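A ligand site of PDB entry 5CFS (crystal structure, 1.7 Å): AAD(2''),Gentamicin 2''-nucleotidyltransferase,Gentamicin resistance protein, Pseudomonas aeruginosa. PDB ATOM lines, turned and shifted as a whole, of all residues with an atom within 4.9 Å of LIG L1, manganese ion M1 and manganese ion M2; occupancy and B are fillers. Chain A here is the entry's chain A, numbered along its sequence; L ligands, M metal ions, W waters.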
ATOM      1  N   GLY A  35     -21.583  14.350 -25.156  1.00  0.00           N
ATOM      2  CA  GLY A  35     -22.171  15.176 -24.120  1.00  0.00           C
ATOM      3  C   GLY A  35     -21.988  16.666 -24.310  1.00  0.00           C
ATOM      4  O   GLY A  35     -22.070  17.191 -25.423  1.00  0.00           O
ATOM      5  N   GLY A  36     -21.732  17.363 -23.212  1.00  0.00           N
ATOM      6  CA  GLY A  36     -21.697  18.807 -23.235  1.00  0.00           C
ATOM      7  C   GLY A  36     -20.624  19.363 -24.134  1.00  0.00           C
ATOM      8  O   GLY A  36     -20.865  20.340 -24.848  1.00  0.00           O
ATOM      9  N   TRP A  37     -19.433  18.771 -24.123  1.00  0.00           N
ATOM     10  CA  TRP A  37     -18.387  19.254 -25.013  1.00  0.00           C
ATOM     11  C   TRP A  37     -18.746  19.017 -26.484  1.00  0.00           C
ATOM     12  O   TRP A  37     -18.322  19.775 -27.352  1.00  0.00           O
ATOM     13  CB  TRP A  37     -17.027  18.608 -24.682  1.00  0.00           C
ATOM     14  CG  TRP A  37     -16.225  19.420 -23.741  1.00  0.00           C
ATOM     15  CD1 TRP A  37     -15.889  19.117 -22.456  1.00  0.00           C
ATOM     16  CD2 TRP A  37     -15.651  20.695 -24.021  1.00  0.00           C
ATOM     17  NE1 TRP A  37     -15.139  20.131 -21.913  1.00  0.00           N
ATOM     18  CE2 TRP A  37     -14.984  21.108 -22.852  1.00  0.00           C
ATOM     19  CE3 TRP A  37     -15.647  21.527 -25.137  1.00  0.00           C
ATOM     20  CZ2 TRP A  37     -14.308  22.327 -22.786  1.00  0.00           C
ATOM     21  CZ3 TRP A  37     -14.980  22.737 -25.071  1.00  0.00           C
ATOM     22  CH2 TRP A  37     -14.311  23.127 -23.898  1.00  0.00           C
ATOM     23  N   ARG A  48     -20.309  27.086 -21.607  1.00  0.00           N
ATOM     24  CA  ARG A  48     -20.248  27.039 -20.154  1.00  0.00           C
ATOM     25  C   ARG A  48     -19.089  26.164 -19.693  1.00  0.00           C
ATOM     26  O   ARG A  48     -18.386  25.566 -20.500  1.00  0.00           O
ATOM     27  CB  ARG A  48     -21.551  26.509 -19.570  1.00  0.00           C
ATOM     28  CG  ARG A  48     -21.920  25.118 -20.071  1.00  0.00           C
ATOM     29  CD  ARG A  48     -23.178  24.624 -19.370  1.00  0.00           C
ATOM     30  NE  ARG A  48     -23.689  23.366 -19.896  1.00  0.00           N
ATOM     31  CZ  ARG A  48     -23.271  22.158 -19.517  1.00  0.00           C
ATOM     32  NH1 ARG A  48     -23.812  21.073 -20.053  1.00  0.00           N
ATOM     33  NH2 ARG A  48     -22.304  22.016 -18.610  1.00  0.00           N
ATOM     34  N   LYS A  49     -18.898  26.094 -18.377  1.00  0.00           N
ATOM     35  CA  LYS A  49     -17.947  25.169 -17.793  1.00  0.00           C
ATOM     36  C   LYS A  49     -18.525  23.766 -17.867  1.00  0.00           C
ATOM     37  O   LYS A  49     -19.735  23.570 -17.707  1.00  0.00           O
ATOM     38  CB  LYS A  49     -17.612  25.550 -16.345  1.00  0.00           C
ATOM     39  CG  LYS A  49     -16.803  26.833 -16.211  1.00  0.00           C
ATOM     40  N   HIS A  50     -17.661  22.796 -18.116  1.00  0.00           N
ATOM     41  CA  HIS A  50     -18.049  21.396 -18.253  1.00  0.00           C
ATOM     42  C   HIS A  50     -17.482  20.557 -17.131  1.00  0.00           C
ATOM     43  O   HIS A  50     -16.292  20.642 -16.824  1.00  0.00           O
ATOM     44  CB  HIS A  50     -17.582  20.860 -19.609  1.00  0.00           C
ATOM     45  CG  HIS A  50     -18.141  21.626 -20.770  1.00  0.00           C
ATOM     46  ND1 HIS A  50     -19.441  21.471 -21.201  1.00  0.00           N
ATOM     47  CD2 HIS A  50     -17.594  22.579 -21.558  1.00  0.00           C
ATOM     48  CE1 HIS A  50     -19.655  22.271 -22.219  1.00  0.00           C
ATOM     49  NE2 HIS A  50     -18.555  22.959 -22.458  1.00  0.00           N
ATOM     50  N   ASP A  51     -18.326  19.731 -16.521  1.00  0.00           N
ATOM     51  CA  ASP A  51     -17.920  18.991 -15.336  1.00  0.00           C
ATOM     52  C   ASP A  51     -17.007  17.822 -15.669  1.00  0.00           C
ATOM     53  O   ASP A  51     -16.149  17.468 -14.866  1.00  0.00           O
ATOM     54  CB  ASP A  51     -19.145  18.477 -14.576  1.00  0.00           C
ATOM     55  CG  ASP A  51     -19.907  19.593 -13.883  1.00  0.00           C
ATOM     56  OD1 ASP A  51     -19.342  20.685 -13.702  1.00  0.00           O
ATOM     57  OD2 ASP A  51     -21.082  19.362 -13.502  1.00  0.00           O
ATOM     58  N   ASP A  52     -17.197  17.224 -16.840  1.00  0.00           N
ATOM     59  CA  ASP A  52     -16.323  16.146 -17.296  1.00  0.00           C
ATOM     60  C   ASP A  52     -16.115  16.227 -18.801  1.00  0.00           C
ATOM     61  O   ASP A  52     -16.601  17.145 -19.459  1.00  0.00           O
ATOM     62  CB  ASP A  52     -16.874  14.757 -16.883  1.00  0.00           C
ATOM     63  CG  ASP A  52     -18.198  14.403 -17.559  1.00  0.00           C
ATOM     64  OD1 ASP A  52     -18.543  15.034 -18.567  1.00  0.00           O
ATOM     65  OD2 ASP A  52     -18.885  13.463 -17.104  1.00  0.00           O
ATOM     66  N   ASP A  54     -16.851  13.724 -21.937  1.00  0.00           N
ATOM     67  CA  ASP A  54     -17.473  12.467 -22.362  1.00  0.00           C
ATOM     68  C   ASP A  54     -16.826  12.015 -23.661  1.00  0.00           C
ATOM     69  O   ASP A  54     -16.723  12.791 -24.610  1.00  0.00           O
ATOM     70  CB  ASP A  54     -18.978  12.636 -22.552  1.00  0.00           C
ATOM     71  CG  ASP A  54     -19.688  13.097 -21.303  1.00  0.00           C
ATOM     72  OD1 ASP A  54     -19.770  12.323 -20.328  1.00  0.00           O
ATOM     73  OD2 ASP A  54     -20.164  14.248 -21.284  1.00  0.00           O
ATOM     74  N   ASP A  94     -15.375  10.340 -19.049  1.00  0.00           N
ATOM     75  CA  ASP A  94     -16.530   9.470 -18.993  1.00  0.00           C
ATOM     76  C   ASP A  94     -16.627   8.733 -20.323  1.00  0.00           C
ATOM     77  O   ASP A  94     -17.064   9.307 -21.324  1.00  0.00           O
ATOM     78  CB  ASP A  94     -17.761  10.332 -18.699  1.00  0.00           C
ATOM     79  CG  ASP A  94     -19.026   9.541 -18.562  1.00  0.00           C
ATOM     80  OD1 ASP A  94     -19.006   8.297 -18.632  1.00  0.00           O
ATOM     81  OD2 ASP A  94     -20.065  10.200 -18.343  1.00  0.00           O
ATOM     82  N   ILE A 136     -26.523  12.619 -29.227  1.00  0.00           N
ATOM     83  CA  ILE A 136     -26.459  13.505 -28.082  1.00  0.00           C
ATOM     84  C   ILE A 136     -27.831  13.648 -27.458  1.00  0.00           C
ATOM     85  O   ILE A 136     -27.985  13.556 -26.258  1.00  0.00           O
ATOM     86  CB  ILE A 136     -25.933  14.890 -28.476  1.00  0.00           C
ATOM     87  CG1 ILE A 136     -24.464  14.787 -28.901  1.00  0.00           C
ATOM     88  CG2 ILE A 136     -26.061  15.884 -27.321  1.00  0.00           C
ATOM     89  CD1 ILE A 136     -23.948  16.010 -29.635  1.00  0.00           C
ATOM     90  N   ASP A 139     -29.485  10.499 -25.541  1.00  0.00           N
ATOM     91  CA  ASP A 139     -29.152  10.248 -24.148  1.00  0.00           C
ATOM     92  C   ASP A 139     -30.026  11.046 -23.187  1.00  0.00           C
ATOM     93  O   ASP A 139     -30.229  10.612 -22.055  1.00  0.00           O
ATOM     94  CB  ASP A 139     -27.664  10.530 -23.886  1.00  0.00           C
ATOM     95  CG  ASP A 139     -26.788   9.314 -24.152  1.00  0.00           C
ATOM     96  OD1 ASP A 139     -27.348   8.201 -24.297  1.00  0.00           O
ATOM     97  OD2 ASP A 139     -25.552   9.463 -24.191  1.00  0.00           O
ATOM     98  N   TYR A 140     -30.563  12.188 -23.629  1.00  0.00           N
ATOM     99  CA  TYR A 140     -31.506  12.924 -22.795  1.00  0.00           C
ATOM    100  C   TYR A 140     -32.806  12.160 -22.635  1.00  0.00           C
ATOM    101  O   TYR A 140     -33.493  12.314 -21.629  1.00  0.00           O
ATOM    102  CB  TYR A 140     -31.791  14.313 -23.371  1.00  0.00           C
ATOM    103  CG  TYR A 140     -30.663  15.296 -23.156  1.00  0.00           C
ATOM    104  CD1 TYR A 140     -30.535  15.999 -21.971  1.00  0.00           C
ATOM    105  CD2 TYR A 140     -29.738  15.528 -24.156  1.00  0.00           C
ATOM    106  CE1 TYR A 140     -29.488  16.890 -21.776  1.00  0.00           C
ATOM    107  CE2 TYR A 140     -28.708  16.415 -23.978  1.00  0.00           C
ATOM    108  CZ  TYR A 140     -28.582  17.089 -22.802  1.00  0.00           C
ATOM    109  OH  TYR A 140     -27.536  17.966 -22.667  1.00  0.00           O
ATOM    110  N   TYR A 142     -33.140   8.866 -22.334  1.00  0.00           N
ATOM    111  CA  TYR A 142     -32.905   7.951 -21.215  1.00  0.00           C
ATOM    112  C   TYR A 142     -33.019   8.661 -19.877  1.00  0.00           C
ATOM    113  O   TYR A 142     -33.599   8.153 -18.922  1.00  0.00           O
ATOM    114  CB  TYR A 142     -31.519   7.314 -21.285  1.00  0.00           C
ATOM    115  CG  TYR A 142     -31.319   6.311 -22.393  1.00  0.00           C
ATOM    116  CD1 TYR A 142     -32.010   5.121 -22.410  1.00  0.00           C
ATOM    117  CD2 TYR A 142     -30.380   6.550 -23.385  1.00  0.00           C
ATOM    118  CE1 TYR A 142     -31.800   4.200 -23.405  1.00  0.00           C
ATOM    119  CE2 TYR A 142     -30.160   5.649 -24.379  1.00  0.00           C
ATOM    120  CZ  TYR A 142     -30.868   4.477 -24.383  1.00  0.00           C
ATOM    121  OH  TYR A 142     -30.655   3.553 -25.369  1.00  0.00           O
ATOM    122  N   TYR A 143     -32.421   9.849 -19.824  1.00  0.00           N
ATOM    123  CA  TYR A 143     -32.437  10.661 -18.614  1.00  0.00           C
ATOM    124  C   TYR A 143     -33.858  11.028 -18.213  1.00  0.00           C
ATOM    125  O   TYR A 143     -34.214  10.938 -17.034  1.00  0.00           O
ATOM    126  CB  TYR A 143     -31.597  11.932 -18.844  1.00  0.00           C
ATOM    127  CG  TYR A 143     -31.358  12.789 -17.610  1.00  0.00           C
ATOM    128  CD1 TYR A 143     -31.281  12.232 -16.348  1.00  0.00           C
ATOM    129  CD2 TYR A 143     -31.179  14.157 -17.737  1.00  0.00           C
ATOM    130  CE1 TYR A 143     -31.050  13.026 -15.220  1.00  0.00           C
ATOM    131  CE2 TYR A 143     -30.954  14.957 -16.627  1.00  0.00           C
ATOM    132  CZ  TYR A 143     -30.883  14.384 -15.379  1.00  0.00           C
ATOM    133  OH  TYR A 143     -30.653  15.178 -14.285  1.00  0.00           O
ATOM    134  N   GLU A 146     -35.690   8.421 -16.243  1.00  0.00           N
ATOM    135  CA  GLU A 146     -35.322   8.309 -14.831  1.00  0.00           C
ATOM    136  C   GLU A 146     -35.844   9.502 -14.040  1.00  0.00           C
ATOM    137  O   GLU A 146     -36.407   9.342 -12.959  1.00  0.00           O
ATOM    138  CB  GLU A 146     -33.807   8.210 -14.668  1.00  0.00           C
ATOM    139  CG  GLU A 146     -33.135   7.132 -15.504  1.00  0.00           C
ATOM    140  CD  GLU A 146     -33.490   5.729 -15.060  1.00  0.00           C
ATOM    141  OE1 GLU A 146     -32.912   5.265 -14.046  1.00  0.00           O
ATOM    142  OE2 GLU A 146     -34.346   5.099 -15.708  1.00  0.00           O
ATOM    143  N   LYS A 155     -28.741  23.438 -15.902  1.00  0.00           N
ATOM    144  CA  LYS A 155     -27.662  22.985 -16.778  1.00  0.00           C
ATOM    145  C   LYS A 155     -28.145  22.056 -17.872  1.00  0.00           C
ATOM    146  O   LYS A 155     -27.859  22.257 -19.055  1.00  0.00           O
ATOM    147  CB  LYS A 155     -26.597  22.224 -15.997  1.00  0.00           C
ATOM    148  CG  LYS A 155     -25.406  23.025 -15.495  1.00  0.00           C
ATOM    149  CD  LYS A 155     -24.280  22.100 -14.958  1.00  0.00           C
ATOM    150  CE  LYS A 155     -24.010  20.897 -15.900  1.00  0.00           C
ATOM    151  NZ  LYS A 155     -22.859  20.037 -15.487  1.00  0.00           N
ATOM    152  N   HIS A 156     -28.833  20.991 -17.457  1.00  0.00           N
ATOM    153  CA  HIS A 156     -29.271  19.940 -18.360  1.00  0.00           C
ATOM    154  C   HIS A 156     -30.435  20.430 -19.223  1.00  0.00           C
ATOM    155  O   HIS A 156     -30.547  20.067 -20.395  1.00  0.00           O
ATOM    156  CB  HIS A 156     -29.672  18.694 -17.578  1.00  0.00           C
ATOM    157  CG  HIS A 156     -28.537  18.029 -16.861  1.00  0.00           C
ATOM    158  ND1 HIS A 156     -28.640  17.609 -15.552  1.00  0.00           N
ATOM    159  CD2 HIS A 156     -27.287  17.707 -17.259  1.00  0.00           C
ATOM    160  CE1 HIS A 156     -27.490  17.061 -15.173  1.00  0.00           C
ATOM    161  NE2 HIS A 156     -26.665  17.099 -16.196  1.00  0.00           N
ATOM    162  N   SER A 159     -28.856  22.761 -21.866  1.00  0.00           N
ATOM    163  CA  SER A 159     -28.059  22.001 -22.829  1.00  0.00           C
ATOM    164  C   SER A 159     -28.967  21.255 -23.785  1.00  0.00           C
ATOM    165  O   SER A 159     -28.728  21.239 -24.997  1.00  0.00           O
ATOM    166  CB  SER A 159     -27.123  21.031 -22.119  1.00  0.00           C
ATOM    167  OG  SER A 159     -26.050  21.729 -21.514  1.00  0.00           O
HETATM  168  P1  LIG L   1     -21.021  18.786 -18.672  1.00  0.00           P
HETATM  169  O1  LIG L   1     -21.008  19.762 -17.568  1.00  0.00           O
HETATM  170  O2  LIG L   1     -20.517  17.392 -18.252  1.00  0.00           O
HETATM  171  O3  LIG L   1     -20.262  19.169 -19.895  1.00  0.00           O
HETATM  172  P2  LIG L   1     -23.199  17.272 -19.751  1.00  0.00           P
HETATM  173  O4  LIG L   1     -24.308  17.594 -20.734  1.00  0.00           O
HETATM  174  O5  LIG L   1     -22.101  16.446 -20.496  1.00  0.00           O
HETATM  175  O6  LIG L   1     -22.506  18.587 -19.223  1.00  0.00           O
HETATM  176  P3  LIG L   1     -23.316  14.669 -18.035  1.00  0.00           P
HETATM  177  O7  LIG L   1     -23.404  14.164 -16.612  1.00  0.00           O
HETATM  178  O8  LIG L   1     -21.831  14.418 -18.458  1.00  0.00           O
HETATM  179  C1  LIG L   1     -23.669  16.415 -18.233  1.00  0.00           C
HETATM  180  O9  LIG L   1     -24.224  13.822 -19.001  1.00  0.00           O
HETATM  181  C2  LIG L   1     -24.736  14.309 -20.258  1.00  0.00           C
HETATM  182  C3  LIG L   1     -25.740  13.324 -20.792  1.00  0.00           C
HETATM  183  O10 LIG L   1     -25.956  12.259 -19.823  1.00  0.00           O
HETATM  184  C4  LIG L   1     -27.120  13.903 -21.069  1.00  0.00           C
HETATM  185  O11 LIG L   1     -27.770  13.180 -22.108  1.00  0.00           O
HETATM  186  C5  LIG L   1     -27.833  13.654 -19.743  1.00  0.00           C
HETATM  187  O12 LIG L   1     -29.243  13.637 -19.895  1.00  0.00           O
HETATM  188  C6  LIG L   1     -27.312  12.265 -19.418  1.00  0.00           C
HETATM  189  N1  LIG L   1     -27.397  11.917 -18.002  1.00  0.00           N
HETATM  190  C7  LIG L   1     -26.972  12.661 -16.934  1.00  0.00           C
HETATM  191  N2  LIG L   1     -27.242  12.137 -15.760  1.00  0.00           N
HETATM  192  C8  LIG L   1     -27.894  10.960 -16.091  1.00  0.00           C
HETATM  193  C9  LIG L   1     -28.478   9.955 -15.294  1.00  0.00           C
HETATM  194  N3  LIG L   1     -28.463   9.954 -13.953  1.00  0.00           N
HETATM  195  N4  LIG L   1     -29.092   8.925 -15.929  1.00  0.00           N
HETATM  196  C10 LIG L   1     -29.096   8.913 -17.268  1.00  0.00           C
HETATM  197  N5  LIG L   1     -28.570   9.792 -18.116  1.00  0.00           N
HETATM  198  C11 LIG L   1     -27.991  10.808 -17.459  1.00  0.00           C
HETATM  199  C1  LG2 L   2     -27.170   5.892 -21.907  1.00  0.00           C
HETATM  200  O1  LG2 L   2     -25.946   6.015 -21.231  1.00  0.00           O
HETATM  201  C2  LG2 L   2     -28.161   5.258 -20.942  1.00  0.00           C
HETATM  202  N1  LG2 L   2     -28.259   6.046 -19.697  1.00  0.00           N
HETATM  203  C3  LG2 L   2     -27.726   3.830 -20.674  1.00  0.00           C
HETATM  204  C4  LG2 L   2     -27.590   3.030 -21.960  1.00  0.00           C
HETATM  205  O2  LG2 L   2     -27.102   1.721 -21.686  1.00  0.00           O
HETATM  206  C5  LG2 L   2     -26.624   3.743 -22.902  1.00  0.00           C
HETATM  207  O3  LG2 L   2     -27.016   5.124 -23.090  1.00  0.00           O
HETATM  208  C6  LG2 L   2     -26.595   3.077 -24.260  1.00  0.00           C
HETATM  209  N2  LG2 L   2     -25.763   3.762 -25.247  1.00  0.00           N
HETATM  210  C7  LG2 L   2     -22.694   8.519 -20.710  1.00  0.00           C
HETATM  211  N3  LG2 L   2     -21.714   9.621 -20.646  1.00  0.00           N
HETATM  212  C8  LG2 L   2     -23.129   8.271 -22.155  1.00  0.00           C
HETATM  213  C9  LG2 L   2     -24.087   7.076 -22.225  1.00  0.00           C
HETATM  214  N4  LG2 L   2     -24.561   6.894 -23.599  1.00  0.00           N
HETATM  215  C10 LG2 L   2     -25.280   7.285 -21.302  1.00  0.00           C
HETATM  216  C11 LG2 L   2     -24.887   7.645 -19.873  1.00  0.00           C
HETATM  217  O4  LG2 L   2     -26.065   7.984 -19.150  1.00  0.00           O
HETATM  218  C12 LG2 L   2     -23.941   8.835 -19.890  1.00  0.00           C
HETATM  219  O5  LG2 L   2     -23.552   9.092 -18.536  1.00  0.00           O
HETATM  220  C13 LG2 L   2     -24.375   9.979 -17.825  1.00  0.00           C
HETATM  221  C14 LG2 L   2     -23.523  11.180 -17.419  1.00  0.00           C
HETATM  222  O6  LG2 L   2     -22.916  11.745 -18.579  1.00  0.00           O
HETATM  223  C15 LG2 L   2     -22.434  10.747 -16.441  1.00  0.00           C
HETATM  224  N5  LG2 L   2     -21.611  11.887 -16.033  1.00  0.00           N
HETATM  225  C16 LG2 L   2     -23.120  10.094 -15.244  1.00  0.00           C
HETATM  226  O7  LG2 L   2     -22.135   9.662 -14.314  1.00  0.00           O
HETATM  227  C17 LG2 L   2     -23.924   8.895 -15.746  1.00  0.00           C
HETATM  228  O8  LG2 L   2     -24.915   9.343 -16.691  1.00  0.00           O
HETATM  229  C18 LG2 L   2     -24.662   8.175 -14.662  1.00  0.00           C
HETATM  230  O9  LG2 L   2     -25.450   7.109 -15.195  1.00  0.00           O
HETATM  231 MN    MN M   1     -20.365  15.539 -19.545  1.00  0.00          MN
HETATM  232 MN    MN M   2     -20.457  12.438 -18.245  1.00  0.00          MN
HETATM  233  O   HOH W   1     -25.242  16.610 -23.216  1.00  0.00           O
HETATM  234  O   HOH W   2     -26.111  13.851 -24.337  1.00  0.00           O
HETATM  235  O   HOH W   3     -28.497   8.877 -20.761  1.00  0.00           O
HETATM  236  O   HOH W   4     -21.053  15.998 -15.533  1.00  0.00           O
HETATM  237  O   HOH W   5     -19.060  17.082 -20.603  1.00  0.00           O
HETATM  238  O   HOH W   6     -26.553  18.439 -20.235  1.00  0.00           O
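The side-chain carboxylate (OD1) of Asp 52 is bound to manganese ion M1, at 2.1 Å. O8 of LIG L1 binds manganese ion M1 (2.1 Å). The side-chain carboxylate (OD2) of Asp 54 is bound to manganese ion M1 (2.2 Å). O5 of LIG L1 binds manganese ion M1, at 2.2 Å. O2 of LIG L1 binds manganese ion M1 (2.3 Å). Manganese ion M1 is bound by water W5, at 2.3 Å. Manganese ion M1 has six donor atoms within binding distance.
Manganese ion M2 is bound by OD2 of Asp 52, OD1 of Asp 54, OD2 of Asp 94, O8 of LIG L1, N5 of LG2 L2 and O6 of LG2 L2. Manganese ion M2 has six donor atoms within binding distance.
Gly 35 touches LIG L1 (C to O5, 3.8 Å). Asp 139 touches LIG L1 (CB to O11, 3.2 Å). Tyr 143 touches LIG L1. NE2 of His 156 touches C1 of LIG L1, 3.7 Å away. Hydrophobic or aromatic side chains within 4 Å of LIG L1: His 50, Tyr 140, Tyr 143 and His 156. Within 4 Å of LIG L1: Gly 35, Gly 36, Arg 48, His 50, Asp 51, Asp 52, Asp 54, Asp 139, Tyr 140, Tyr 143, Lys 155 and His 156. Along chain A the residues within 4 Å of LIG L1 span positions 35 to 156. The nearest printed residue that does not touch LIG L1 is Lys 49 (4.02 Å).
Within 4 Å of manganese ion M1: Asp 52 and Asp 54. The nearest printed residue that does not touch manganese ion M1 is Gly 36 (4.3 Å).
ND1 of His 50 sits at hydrogen-bond distance from O3 of LIG L1 (2.8 Å). O1 of LIG L1 is in salt-bridge range of NZ of Lys 155 (2.8 Å). O1 of LIG L1 lies within salt-bridge range of NH2 of Arg 48 (2.8 Å). The backbone NH of Asp 51 lies within hydrogen-bond range of an oxygen (O1) of LIG L1, 2.9 Å away. The backbone NH of Gly 36 lies close to an oxygen (O5) of LIG L1. An oxygen (O11) of LIG L1 is in hydrogen-bond range of the backbone NH (N) of Tyr 140, at 3.3 Å. OD2 of Asp 139 is in salt-bridge range of N4 of LG2 L2, 2.8 Å away.
Of the 19 residues printed, 3 come within 4 Å of manganese ion M2.
Water W5 lies within hydrogen-bond range of O3 of LIG L1 (2.5 Å) and O of Asp 52 (2.7 Å). Water W6 bridges an oxygen (O4) of LIG L1 and the side-chain hydroxyl of Tyr 140. Water W3 lies within hydrogen-bond range of O of Asp 139 (2.8 Å), N5 of LIG L1 (2.8 Å) and N1 of LG2 L2 (3.0 Å). Water W1 lies within hydrogen-bond range of OH of Tyr 140 (2.7 Å) and O4 of LIG L1 (2.8 Å). Water W2 bridges the backbone carbonyl oxygen (O) of Ile 136 and an oxygen (O11) of LIG L1.
A ring nitrogen (NE2) of His 50 is in hydrogen-bond range of the backbone carbonyl oxygen (O) of Arg 48 (3.3 Å). OD2 of Asp 51 is in salt-bridge range of NZ of Lys 155, at 2.7 Å. The backbone carbonyl oxygen of Lys 155 sits at hydrogen-bond distance from the side-chain hydroxyl of Ser 159 (3.1 Å). OG of Ser 159 is in hydrogen-bond range of NH1 of Arg 48, at 2.8 Å. OH of Tyr 143 sits at hydrogen-bond distance from ND1 of His 156, at 3.4 Å.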
